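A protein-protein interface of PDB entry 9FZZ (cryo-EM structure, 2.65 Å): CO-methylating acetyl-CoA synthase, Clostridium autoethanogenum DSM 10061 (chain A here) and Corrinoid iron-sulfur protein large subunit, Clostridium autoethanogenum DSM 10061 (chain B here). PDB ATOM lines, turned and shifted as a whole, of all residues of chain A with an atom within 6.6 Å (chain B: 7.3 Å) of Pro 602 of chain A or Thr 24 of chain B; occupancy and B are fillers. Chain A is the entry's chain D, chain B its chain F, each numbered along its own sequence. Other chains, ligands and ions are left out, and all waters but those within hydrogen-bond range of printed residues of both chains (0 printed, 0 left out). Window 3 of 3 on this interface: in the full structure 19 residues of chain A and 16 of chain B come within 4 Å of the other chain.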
ATOM      1  N   MET A 584      -6.943  19.969  -0.699  1.00  0.00           N
ATOM      2  CA  MET A 584      -6.995  18.519  -0.561  1.00  0.00           C
ATOM      3  C   MET A 584      -5.604  18.017  -0.215  1.00  0.00           C
ATOM      4  O   MET A 584      -4.714  18.024  -1.085  1.00  0.00           O
ATOM      5  CB  MET A 584      -7.499  17.872  -1.850  1.00  0.00           C
ATOM      6  CG  MET A 584      -7.932  16.421  -1.666  1.00  0.00           C
ATOM      7  SD  MET A 584      -9.032  15.901  -2.998  1.00  0.00           S
ATOM      8  CE  MET A 584      -8.437  14.262  -3.359  1.00  0.00           C
ATOM      9  N   GLU A 586      -4.379  14.897   0.770  1.00  0.00           N
ATOM     10  CA  GLU A 586      -3.964  13.591   0.265  1.00  0.00           C
ATOM     11  C   GLU A 586      -3.574  13.654  -1.204  1.00  0.00           C
ATOM     12  O   GLU A 586      -2.740  12.864  -1.654  1.00  0.00           O
ATOM     13  CB  GLU A 586      -5.063  12.544   0.487  1.00  0.00           C
ATOM     14  CG  GLU A 586      -6.339  12.789  -0.315  1.00  0.00           C
ATOM     15  CD  GLU A 586      -7.347  13.612   0.460  1.00  0.00           C
ATOM     16  OE1 GLU A 586      -6.922  14.450   1.275  1.00  0.00           O
ATOM     17  OE2 GLU A 586      -8.563  13.409   0.261  1.00  0.00           O
ATOM     18  N   VAL A 591      -9.098  21.420  -4.770  1.00  0.00           N
ATOM     19  CA  VAL A 591     -10.276  21.140  -5.575  1.00  0.00           C
ATOM     20  C   VAL A 591     -11.137  22.393  -5.592  1.00  0.00           C
ATOM     21  O   VAL A 591     -11.019  23.272  -4.735  1.00  0.00           O
ATOM     22  CB  VAL A 591     -11.094  19.938  -5.059  1.00  0.00           C
ATOM     23  CG1 VAL A 591     -10.174  18.783  -4.700  1.00  0.00           C
ATOM     24  CG2 VAL A 591     -11.951  20.330  -3.867  1.00  0.00           C
ATOM     25  N   MET A 592     -12.026  22.461  -6.574  1.00  0.00           N
ATOM     26  CA  MET A 592     -12.894  23.610  -6.765  1.00  0.00           C
ATOM     27  C   MET A 592     -14.330  23.143  -6.936  1.00  0.00           C
ATOM     28  O   MET A 592     -14.582  22.008  -7.351  1.00  0.00           O
ATOM     29  CB  MET A 592     -12.507  24.421  -7.980  1.00  0.00           C
ATOM     30  CG  MET A 592     -11.132  25.053  -7.896  1.00  0.00           C
ATOM     31  SD  MET A 592     -10.780  25.975  -9.410  1.00  0.00           S
ATOM     32  CE  MET A 592     -12.419  26.522  -9.905  1.00  0.00           C
ATOM     33  N   THR A 600     -21.630  15.772  -4.112  1.00  0.00           N
ATOM     34  CA  THR A 600     -20.539  15.876  -3.157  1.00  0.00           C
ATOM     35  C   THR A 600     -19.221  16.111  -3.895  1.00  0.00           C
ATOM     36  O   THR A 600     -19.120  15.961  -5.113  1.00  0.00           O
ATOM     37  CB  THR A 600     -20.465  14.613  -2.296  1.00  0.00           C
ATOM     38  OG1 THR A 600     -19.439  14.740  -1.302  1.00  0.00           O
ATOM     39  CG2 THR A 600     -20.170  13.390  -3.157  1.00  0.00           C
ATOM     40  N   THR A 601     -18.195  16.485  -3.134  1.00  0.00           N
ATOM     41  CA  THR A 601     -16.863  16.780  -3.625  1.00  0.00           C
ATOM     42  C   THR A 601     -15.857  15.849  -2.964  1.00  0.00           C
ATOM     43  O   THR A 601     -16.142  15.265  -1.910  1.00  0.00           O
ATOM     44  CB  THR A 601     -16.464  18.242  -3.360  1.00  0.00           C
ATOM     45  OG1 THR A 601     -16.482  18.517  -1.952  1.00  0.00           O
ATOM     46  CG2 THR A 601     -17.421  19.186  -4.060  1.00  0.00           C
ATOM     47  N   PRO A 602     -14.672  15.680  -3.552  1.00  0.00           N
ATOM     48  CA  PRO A 602     -13.663  14.814  -2.911  1.00  0.00           C
ATOM     49  C   PRO A 602     -13.286  15.261  -1.514  1.00  0.00           C
ATOM     50  O   PRO A 602     -12.818  14.436  -0.724  1.00  0.00           O
ATOM     51  CB  PRO A 602     -12.471  14.884  -3.876  1.00  0.00           C
ATOM     52  CG  PRO A 602     -13.091  15.190  -5.219  1.00  0.00           C
ATOM     53  CD  PRO A 602     -14.274  16.089  -4.911  1.00  0.00           C
ATOM     54  N   LEU A 603     -13.473  16.536  -1.180  1.00  0.00           N
ATOM     55  CA  LEU A 603     -13.268  16.964   0.196  1.00  0.00           C
ATOM     56  C   LEU A 603     -14.260  16.322   1.155  1.00  0.00           C
ATOM     57  O   LEU A 603     -13.983  16.247   2.356  1.00  0.00           O
ATOM     58  CB  LEU A 603     -13.387  18.487   0.306  1.00  0.00           C
ATOM     59  CG  LEU A 603     -12.356  19.293  -0.487  1.00  0.00           C
ATOM     60  CD1 LEU A 603     -12.585  20.771  -0.263  1.00  0.00           C
ATOM     61  CD2 LEU A 603     -10.936  18.909  -0.091  1.00  0.00           C
ATOM     62  N   GLY A 604     -15.401  15.856   0.660  1.00  0.00           N
ATOM     63  CA  GLY A 604     -16.416  15.275   1.507  1.00  0.00           C
ATOM     64  C   GLY A 604     -17.532  16.210   1.913  1.00  0.00           C
ATOM     65  O   GLY A 604     -18.364  15.825   2.741  1.00  0.00           O
ATOM     66  N   MET A 605     -17.576  17.423   1.364  1.00  0.00           N
ATOM     67  CA  MET A 605     -18.606  18.396   1.686  1.00  0.00           C
ATOM     68  C   MET A 605     -19.184  18.954   0.393  1.00  0.00           C
ATOM     69  O   MET A 605     -18.502  19.023  -0.634  1.00  0.00           O
ATOM     70  CB  MET A 605     -18.050  19.535   2.547  1.00  0.00           C
ATOM     71  CG  MET A 605     -16.952  19.071   3.508  1.00  0.00           C
ATOM     72  SD  MET A 605     -16.199  20.459   4.372  1.00  0.00           S
ATOM     73  CE  MET A 605     -14.540  19.862   4.628  1.00  0.00           C
ATOM     74  N   TRP A 648      -9.159  18.732  -8.994  1.00  0.00           N
ATOM     75  CA  TRP A 648     -10.539  18.317  -9.190  1.00  0.00           C
ATOM     76  C   TRP A 648     -11.389  19.553  -9.449  1.00  0.00           C
ATOM     77  O   TRP A 648     -11.167  20.601  -8.842  1.00  0.00           O
ATOM     78  CB  TRP A 648     -11.066  17.537  -7.975  1.00  0.00           C
ATOM     79  CG  TRP A 648     -12.380  16.835  -8.222  1.00  0.00           C
ATOM     80  CD1 TRP A 648     -12.561  15.532  -8.593  1.00  0.00           C
ATOM     81  CD2 TRP A 648     -13.696  17.397  -8.099  1.00  0.00           C
ATOM     82  NE1 TRP A 648     -13.904  15.253  -8.714  1.00  0.00           N
ATOM     83  CE2 TRP A 648     -14.623  16.390  -8.413  1.00  0.00           C
ATOM     84  CE3 TRP A 648     -14.169  18.677  -7.750  1.00  0.00           C
ATOM     85  CZ2 TRP A 648     -16.006  16.601  -8.395  1.00  0.00           C
ATOM     86  CZ3 TRP A 648     -15.554  18.895  -7.731  1.00  0.00           C
ATOM     87  CH2 TRP A 648     -16.453  17.858  -8.053  1.00  0.00           C
ATOM     88  N   ALA A 684     -14.215  10.630 -11.463  1.00  0.00           N
ATOM     89  CA  ALA A 684     -13.992  10.101 -10.125  1.00  0.00           C
ATOM     90  C   ALA A 684     -14.364  11.170  -9.112  1.00  0.00           C
ATOM     91  O   ALA A 684     -14.016  12.337  -9.296  1.00  0.00           O
ATOM     92  CB  ALA A 684     -12.533   9.658  -9.942  1.00  0.00           C
ATOM     93  N   THR A 685     -15.070  10.768  -8.055  1.00  0.00           N
ATOM     94  CA  THR A 685     -15.444  11.667  -6.974  1.00  0.00           C
ATOM     95  C   THR A 685     -14.883  11.254  -5.622  1.00  0.00           C
ATOM     96  O   THR A 685     -14.570  12.125  -4.812  1.00  0.00           O
ATOM     97  CB  THR A 685     -16.976  11.766  -6.848  1.00  0.00           C
ATOM     98  OG1 THR A 685     -17.574  11.950  -8.140  1.00  0.00           O
ATOM     99  CG2 THR A 685     -17.364  12.938  -5.961  1.00  0.00           C
ATOM    100  N   GLU A 686     -14.764   9.958  -5.354  1.00  0.00           N
ATOM    101  CA  GLU A 686     -14.123   9.495  -4.131  1.00  0.00           C
ATOM    102  C   GLU A 686     -12.648   9.887  -4.133  1.00  0.00           C
ATOM    103  O   GLU A 686     -11.990   9.914  -5.175  1.00  0.00           O
ATOM    104  CB  GLU A 686     -14.289   7.977  -4.002  1.00  0.00           C
ATOM    105  CG  GLU A 686     -13.591   7.345  -2.783  1.00  0.00           C
ATOM    106  CD  GLU A 686     -14.458   7.399  -1.535  1.00  0.00           C
ATOM    107  OE1 GLU A 686     -15.094   8.443  -1.302  1.00  0.00           O
ATOM    108  OE2 GLU A 686     -14.516   6.392  -0.798  1.00  0.00           O
ATOM    109  N   SER A 687     -12.128  10.183  -2.939  1.00  0.00           N
ATOM    110  CA  SER A 687     -10.766  10.693  -2.821  1.00  0.00           C
ATOM    111  C   SER A 687      -9.747   9.692  -3.351  1.00  0.00           C
ATOM    112  O   SER A 687      -8.813  10.068  -4.070  1.00  0.00           O
ATOM    113  CB  SER A 687     -10.481  11.042  -1.352  1.00  0.00           C
ATOM    114  OG  SER A 687      -9.140  11.484  -1.151  1.00  0.00           O
ATOM    115  N   VAL A 690      -9.779   9.701  -7.059  1.00  0.00           N
ATOM    116  CA  VAL A 690      -9.167  10.927  -7.565  1.00  0.00           C
ATOM    117  C   VAL A 690      -7.649  10.814  -7.543  1.00  0.00           C
ATOM    118  O   VAL A 690      -6.972  11.164  -8.516  1.00  0.00           O
ATOM    119  CB  VAL A 690      -9.655  12.137  -6.751  1.00  0.00           C
ATOM    120  CG1 VAL A 690      -8.865  13.389  -7.116  1.00  0.00           C
ATOM    121  CG2 VAL A 690     -11.135  12.367  -7.000  1.00  0.00           C
ATOM    122  N   PHE B   9      -7.072  18.671  11.783  1.00  0.00           N
ATOM    123  CA  PHE B   9      -6.928  17.720  10.682  1.00  0.00           C
ATOM    124  C   PHE B   9      -5.564  17.068  10.699  1.00  0.00           C
ATOM    125  O   PHE B   9      -5.430  15.887  10.357  1.00  0.00           O
ATOM    126  CB  PHE B   9      -7.153  18.375   9.319  1.00  0.00           C
ATOM    127  CG  PHE B   9      -6.922  17.435   8.158  1.00  0.00           C
ATOM    128  CD1 PHE B   9      -7.925  16.554   7.747  1.00  0.00           C
ATOM    129  CD2 PHE B   9      -5.693  17.407   7.498  1.00  0.00           C
ATOM    130  CE1 PHE B   9      -7.718  15.658   6.681  1.00  0.00           C
ATOM    131  CE2 PHE B   9      -5.460  16.519   6.437  1.00  0.00           C
ATOM    132  CZ  PHE B   9      -6.480  15.642   6.023  1.00  0.00           C
ATOM    133  N   LYS B  14      -6.588  10.248   9.275  1.00  0.00           N
ATOM    134  CA  LYS B  14      -6.569  10.410   7.828  1.00  0.00           C
ATOM    135  C   LYS B  14      -6.864   9.102   7.098  1.00  0.00           C
ATOM    136  O   LYS B  14      -6.493   8.946   5.932  1.00  0.00           O
ATOM    137  CB  LYS B  14      -5.230  10.993   7.361  1.00  0.00           C
ATOM    138  CG  LYS B  14      -4.897  12.329   8.036  1.00  0.00           C
ATOM    139  CD  LYS B  14      -3.428  12.711   7.835  1.00  0.00           C
ATOM    140  CE  LYS B  14      -3.079  13.966   8.654  1.00  0.00           C
ATOM    141  NZ  LYS B  14      -1.624  14.328   8.555  1.00  0.00           N
ATOM    142  N   LYS B  15      -7.547   8.160   7.751  1.00  0.00           N
ATOM    143  CA  LYS B  15      -7.902   6.910   7.087  1.00  0.00           C
ATOM    144  C   LYS B  15      -9.054   7.081   6.113  1.00  0.00           C
ATOM    145  O   LYS B  15      -9.173   6.314   5.151  1.00  0.00           O
ATOM    146  CB  LYS B  15      -8.247   5.828   8.118  1.00  0.00           C
ATOM    147  CG  LYS B  15      -7.051   4.941   8.518  1.00  0.00           C
ATOM    148  CD  LYS B  15      -5.996   5.754   9.289  1.00  0.00           C
ATOM    149  CE  LYS B  15      -4.758   4.902   9.628  1.00  0.00           C
ATOM    150  NZ  LYS B  15      -5.126   3.695  10.447  1.00  0.00           N
ATOM    151  N   ASN B  16      -9.908   8.076   6.345  1.00  0.00           N
ATOM    152  CA  ASN B  16     -11.094   8.315   5.526  1.00  0.00           C
ATOM    153  C   ASN B  16     -11.952   7.051   5.454  1.00  0.00           C
ATOM    154  O   ASN B  16     -12.432   6.650   4.393  1.00  0.00           O
ATOM    155  CB  ASN B  16     -10.708   8.796   4.127  1.00  0.00           C
ATOM    156  CG  ASN B  16      -9.977  10.136   4.137  1.00  0.00           C
ATOM    157  OD1 ASN B  16     -10.239  10.975   4.989  1.00  0.00           O
ATOM    158  ND2 ASN B  16      -9.057  10.335   3.195  1.00  0.00           N
ATOM    159  N   CYS B  17     -12.141   6.418   6.614  1.00  0.00           N
ATOM    160  CA  CYS B  17     -12.864   5.153   6.702  1.00  0.00           C
ATOM    161  C   CYS B  17     -14.376   5.333   6.709  1.00  0.00           C
ATOM    162  O   CYS B  17     -15.103   4.336   6.628  1.00  0.00           O
ATOM    163  CB  CYS B  17     -12.424   4.352   7.935  1.00  0.00           C
ATOM    164  SG  CYS B  17     -12.665   5.172   9.482  1.00  0.00           S
ATOM    165  N   LYS B  18     -14.866   6.572   6.800  1.00  0.00           N
ATOM    166  CA  LYS B  18     -16.295   6.868   6.817  1.00  0.00           C
ATOM    167  C   LYS B  18     -17.011   6.230   8.003  1.00  0.00           C
ATOM    168  O   LYS B  18     -18.238   6.077   7.980  1.00  0.00           O
ATOM    169  CB  LYS B  18     -16.975   6.420   5.516  1.00  0.00           C
ATOM    170  CG  LYS B  18     -16.302   6.930   4.244  1.00  0.00           C
ATOM    171  CD  LYS B  18     -17.089   6.487   3.006  1.00  0.00           C
ATOM    172  CE  LYS B  18     -16.385   6.924   1.716  1.00  0.00           C
ATOM    173  NZ  LYS B  18     -16.286   8.423   1.624  1.00  0.00           N
ATOM    174  N   CYS B  20     -17.263   7.499  11.022  1.00  0.00           N
ATOM    175  CA  CYS B  20     -17.878   8.535  11.843  1.00  0.00           C
ATOM    176  C   CYS B  20     -19.100   9.144  11.170  1.00  0.00           C
ATOM    177  O   CYS B  20     -19.647  10.126  11.680  1.00  0.00           O
ATOM    178  CB  CYS B  20     -16.870   9.637  12.197  1.00  0.00           C
ATOM    179  SG  CYS B  20     -16.088  10.399  10.771  1.00  0.00           S
ATOM    180  N   GLY B  21     -19.535   8.593  10.034  1.00  0.00           N
ATOM    181  CA  GLY B  21     -20.625   9.179   9.287  1.00  0.00           C
ATOM    182  C   GLY B  21     -20.214  10.281   8.339  1.00  0.00           C
ATOM    183  O   GLY B  21     -21.061  10.775   7.582  1.00  0.00           O
ATOM    184  N   PHE B  22     -18.943  10.687   8.356  1.00  0.00           N
ATOM    185  CA  PHE B  22     -18.410  11.725   7.492  1.00  0.00           C
ATOM    186  C   PHE B  22     -17.463  11.117   6.474  1.00  0.00           C
ATOM    187  O   PHE B  22     -16.560  10.359   6.852  1.00  0.00           O
ATOM    188  CB  PHE B  22     -17.684  12.781   8.328  1.00  0.00           C
ATOM    189  CG  PHE B  22     -18.550  13.427   9.368  1.00  0.00           C
ATOM    190  CD1 PHE B  22     -19.888  13.723   9.088  1.00  0.00           C
ATOM    191  CD2 PHE B  22     -18.044  13.722  10.630  1.00  0.00           C
ATOM    192  CE1 PHE B  22     -20.714  14.321  10.052  1.00  0.00           C
ATOM    193  CE2 PHE B  22     -18.848  14.320  11.612  1.00  0.00           C
ATOM    194  CZ  PHE B  22     -20.193  14.621  11.322  1.00  0.00           C
ATOM    195  N   PRO B  23     -17.632  11.420   5.183  1.00  0.00           N
ATOM    196  CA  PRO B  23     -16.843  10.706   4.160  1.00  0.00           C
ATOM    197  C   PRO B  23     -15.338  10.871   4.290  1.00  0.00           C
ATOM    198  O   PRO B  23     -14.603   9.928   3.973  1.00  0.00           O
ATOM    199  CB  PRO B  23     -17.372  11.284   2.834  1.00  0.00           C
ATOM    200  CG  PRO B  23     -18.017  12.613   3.206  1.00  0.00           C
ATOM    201  CD  PRO B  23     -18.563  12.403   4.596  1.00  0.00           C
ATOM    202  N   THR B  24     -14.849  12.019   4.754  1.00  0.00           N
ATOM    203  CA  THR B  24     -13.421  12.277   4.835  1.00  0.00           C
ATOM    204  C   THR B  24     -13.052  12.785   6.224  1.00  0.00           C
ATOM    205  O   THR B  24     -13.882  13.334   6.953  1.00  0.00           O
ATOM    206  CB  THR B  24     -12.950  13.281   3.772  1.00  0.00           C
ATOM    207  OG1 THR B  24     -13.893  14.353   3.654  1.00  0.00           O
ATOM    208  CG2 THR B  24     -12.799  12.591   2.428  1.00  0.00           C
ATOM    209  N   CYS B  25     -11.782  12.587   6.579  1.00  0.00           N
ATOM    210  CA  CYS B  25     -11.288  13.099   7.852  1.00  0.00           C
ATOM    211  C   CYS B  25     -11.314  14.616   7.881  1.00  0.00           C
ATOM    212  O   CYS B  25     -11.480  15.212   8.946  1.00  0.00           O
ATOM    213  CB  CYS B  25      -9.858  12.609   8.111  1.00  0.00           C
ATOM    214  SG  CYS B  25      -9.763  11.017   8.958  1.00  0.00           S
ATOM    215  N   LEU B  26     -11.136  15.259   6.726  1.00  0.00           N
ATOM    216  CA  LEU B  26     -11.243  16.711   6.679  1.00  0.00           C
ATOM    217  C   LEU B  26     -12.658  17.161   7.012  1.00  0.00           C
ATOM    218  O   LEU B  26     -12.854  18.158   7.713  1.00  0.00           O
ATOM    219  CB  LEU B  26     -10.827  17.224   5.301  1.00  0.00           C
ATOM    220  CG  LEU B  26     -10.617  18.742   5.206  1.00  0.00           C
ATOM    221  CD1 LEU B  26      -9.168  19.110   5.509  1.00  0.00           C
ATOM    222  CD2 LEU B  26     -11.029  19.238   3.828  1.00  0.00           C
ATOM    223  N   ALA B  27     -13.662  16.439   6.511  1.00  0.00           N
ATOM    224  CA  ALA B  27     -15.047  16.775   6.829  1.00  0.00           C
ATOM    225  C   ALA B  27     -15.321  16.637   8.318  1.00  0.00           C
ATOM    226  O   ALA B  27     -15.950  17.511   8.925  1.00  0.00           O
ATOM    227  CB  ALA B  27     -16.001  15.896   6.018  1.00  0.00           C
ATOM    228  N   PHE B  28     -14.832  15.558   8.927  1.00  0.00           N
ATOM    229  CA  PHE B  28     -14.992  15.383  10.368  1.00  0.00           C
ATOM    230  C   PHE B  28     -14.274  16.488  11.131  1.00  0.00           C
ATOM    231  O   PHE B  28     -14.810  17.035  12.104  1.00  0.00           O
ATOM    232  CB  PHE B  28     -14.475  14.001  10.781  1.00  0.00           C
ATOM    233  CG  PHE B  28     -14.359  13.810  12.269  1.00  0.00           C
ATOM    234  CD1 PHE B  28     -15.479  13.468  13.029  1.00  0.00           C
ATOM    235  CD2 PHE B  28     -13.131  13.974  12.911  1.00  0.00           C
ATOM    236  CE1 PHE B  28     -15.386  13.296  14.421  1.00  0.00           C
ATOM    237  CE2 PHE B  28     -13.010  13.808  14.301  1.00  0.00           C
ATOM    238  CZ  PHE B  28     -14.143  13.467  15.060  1.00  0.00           C
ATOM    239  N   SER B  29     -13.066  16.841  10.694  1.00  0.00           N
ATOM    240  CA  SER B  29     -12.303  17.891  11.357  1.00  0.00           C
ATOM    241  C   SER B  29     -13.032  19.225  11.281  1.00  0.00           C
ATOM    242  O   SER B  29     -13.108  19.959  12.271  1.00  0.00           O
ATOM    243  CB  SER B  29     -10.911  17.967  10.713  1.00  0.00           C
ATOM    244  OG  SER B  29     -10.273  19.214  10.959  1.00  0.00           O
ATOM    245  N   MET B  30     -13.648  19.526  10.146  1.00  0.00           N
ATOM    246  CA  MET B  30     -14.387  20.781  10.045  1.00  0.00           C
ATOM    247  C   MET B  30     -15.685  20.735  10.843  1.00  0.00           C
ATOM    248  O   MET B  30     -16.094  21.751  11.417  1.00  0.00           O
ATOM    249  CB  MET B  30     -14.661  21.109   8.574  1.00  0.00           C
ATOM    250  CG  MET B  30     -13.372  21.380   7.778  1.00  0.00           C
ATOM    251  SD  MET B  30     -12.477  22.824   8.384  1.00  0.00           S
ATOM    252  CE  MET B  30     -10.876  22.616   7.624  1.00  0.00           C
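The backbone carbonyl oxygen (O) of Met 605 of chain A is in hydrogen-bond range of the side-chain hydroxyl (OG1) of Thr 601 of chain A (2.5 Å). NZ of Lys 18 of chain B sits at hydrogen-bond distance from O of Pro 23 of chain B, at 3.3 Å.
The side-chain carboxylate (OE1) of Glu 686 of chain A is in salt-bridge range of the side-chain amino group (NZ) of Lys 18 of chain B (3.2 Å). The side-chain hydroxyl (OG1) of Thr 24 of chain B sits close to the backbone carbonyl oxygen (O) of Leu 603 of chain A (2.3 Å).
O of Pro 602 of chain A touches CG2 of Thr 24 of chain B, 3.7 Å away. Leu 603 of chain A touches Leu 26 of chain B. Gly 604 of chain A touches Pro 23 of chain B. Gly 604 of chain A touches Thr 24 of chain B. Leu 26 of chain B touches Met 605 of chain A (CD2 to CE, 3.7 Å). Ala 27 of chain B touches Met 605 of chain A. Met 605 of chain A touches Met 30 of chain B (CE to CG, 3.7 Å).
Of the 17 printed residues of chain B, 6 touch a printed residue of chain A. Hydrophobic or aromatic side chains of chain B within 4 Å of the printed part of chain A: Pro 23, Leu 26 and Met 30. Printed residues of chain A that touch a printed residue of chain B: Pro 602, Leu 603, Gly 604, Met 605 and Glu 686. Along chain A the printed residues that touch a printed residue of chain B span positions 602 to 686. Among the printed residues, 9 pairs touch across the chains.
Pro 602 of chain A touches just one residue of chain B: Thr 24. Printed residues of chain B within 4 Å of Leu 603 of chain A: Thr 24 (2.3 Å) and Leu 26 (3.9 Å). Printed residues of chain B within 4 Å of Met 605 of chain A: Leu 26 (3.7 Å), Ala 27 (3.8 Å) and Met 30 (3.7 Å). Cys 17 of chain B touches none of the printed residues of chain A. Of the printed residues of chain A, Pro 23 of chain B touches Gly 604 (3.3 Å). Of chain A, only Pro 602, Leu 603 and Gly 604 come within 4 Å of Thr 24 of chain B. The nearest residue of chain B that does not touch Pro 602 of chain A is Pro 23 of chain B (6.6 Å). The nearest residue of chain A that does not touch Thr 24 of chain B is Ser 687 of chain A (4.7 Å).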
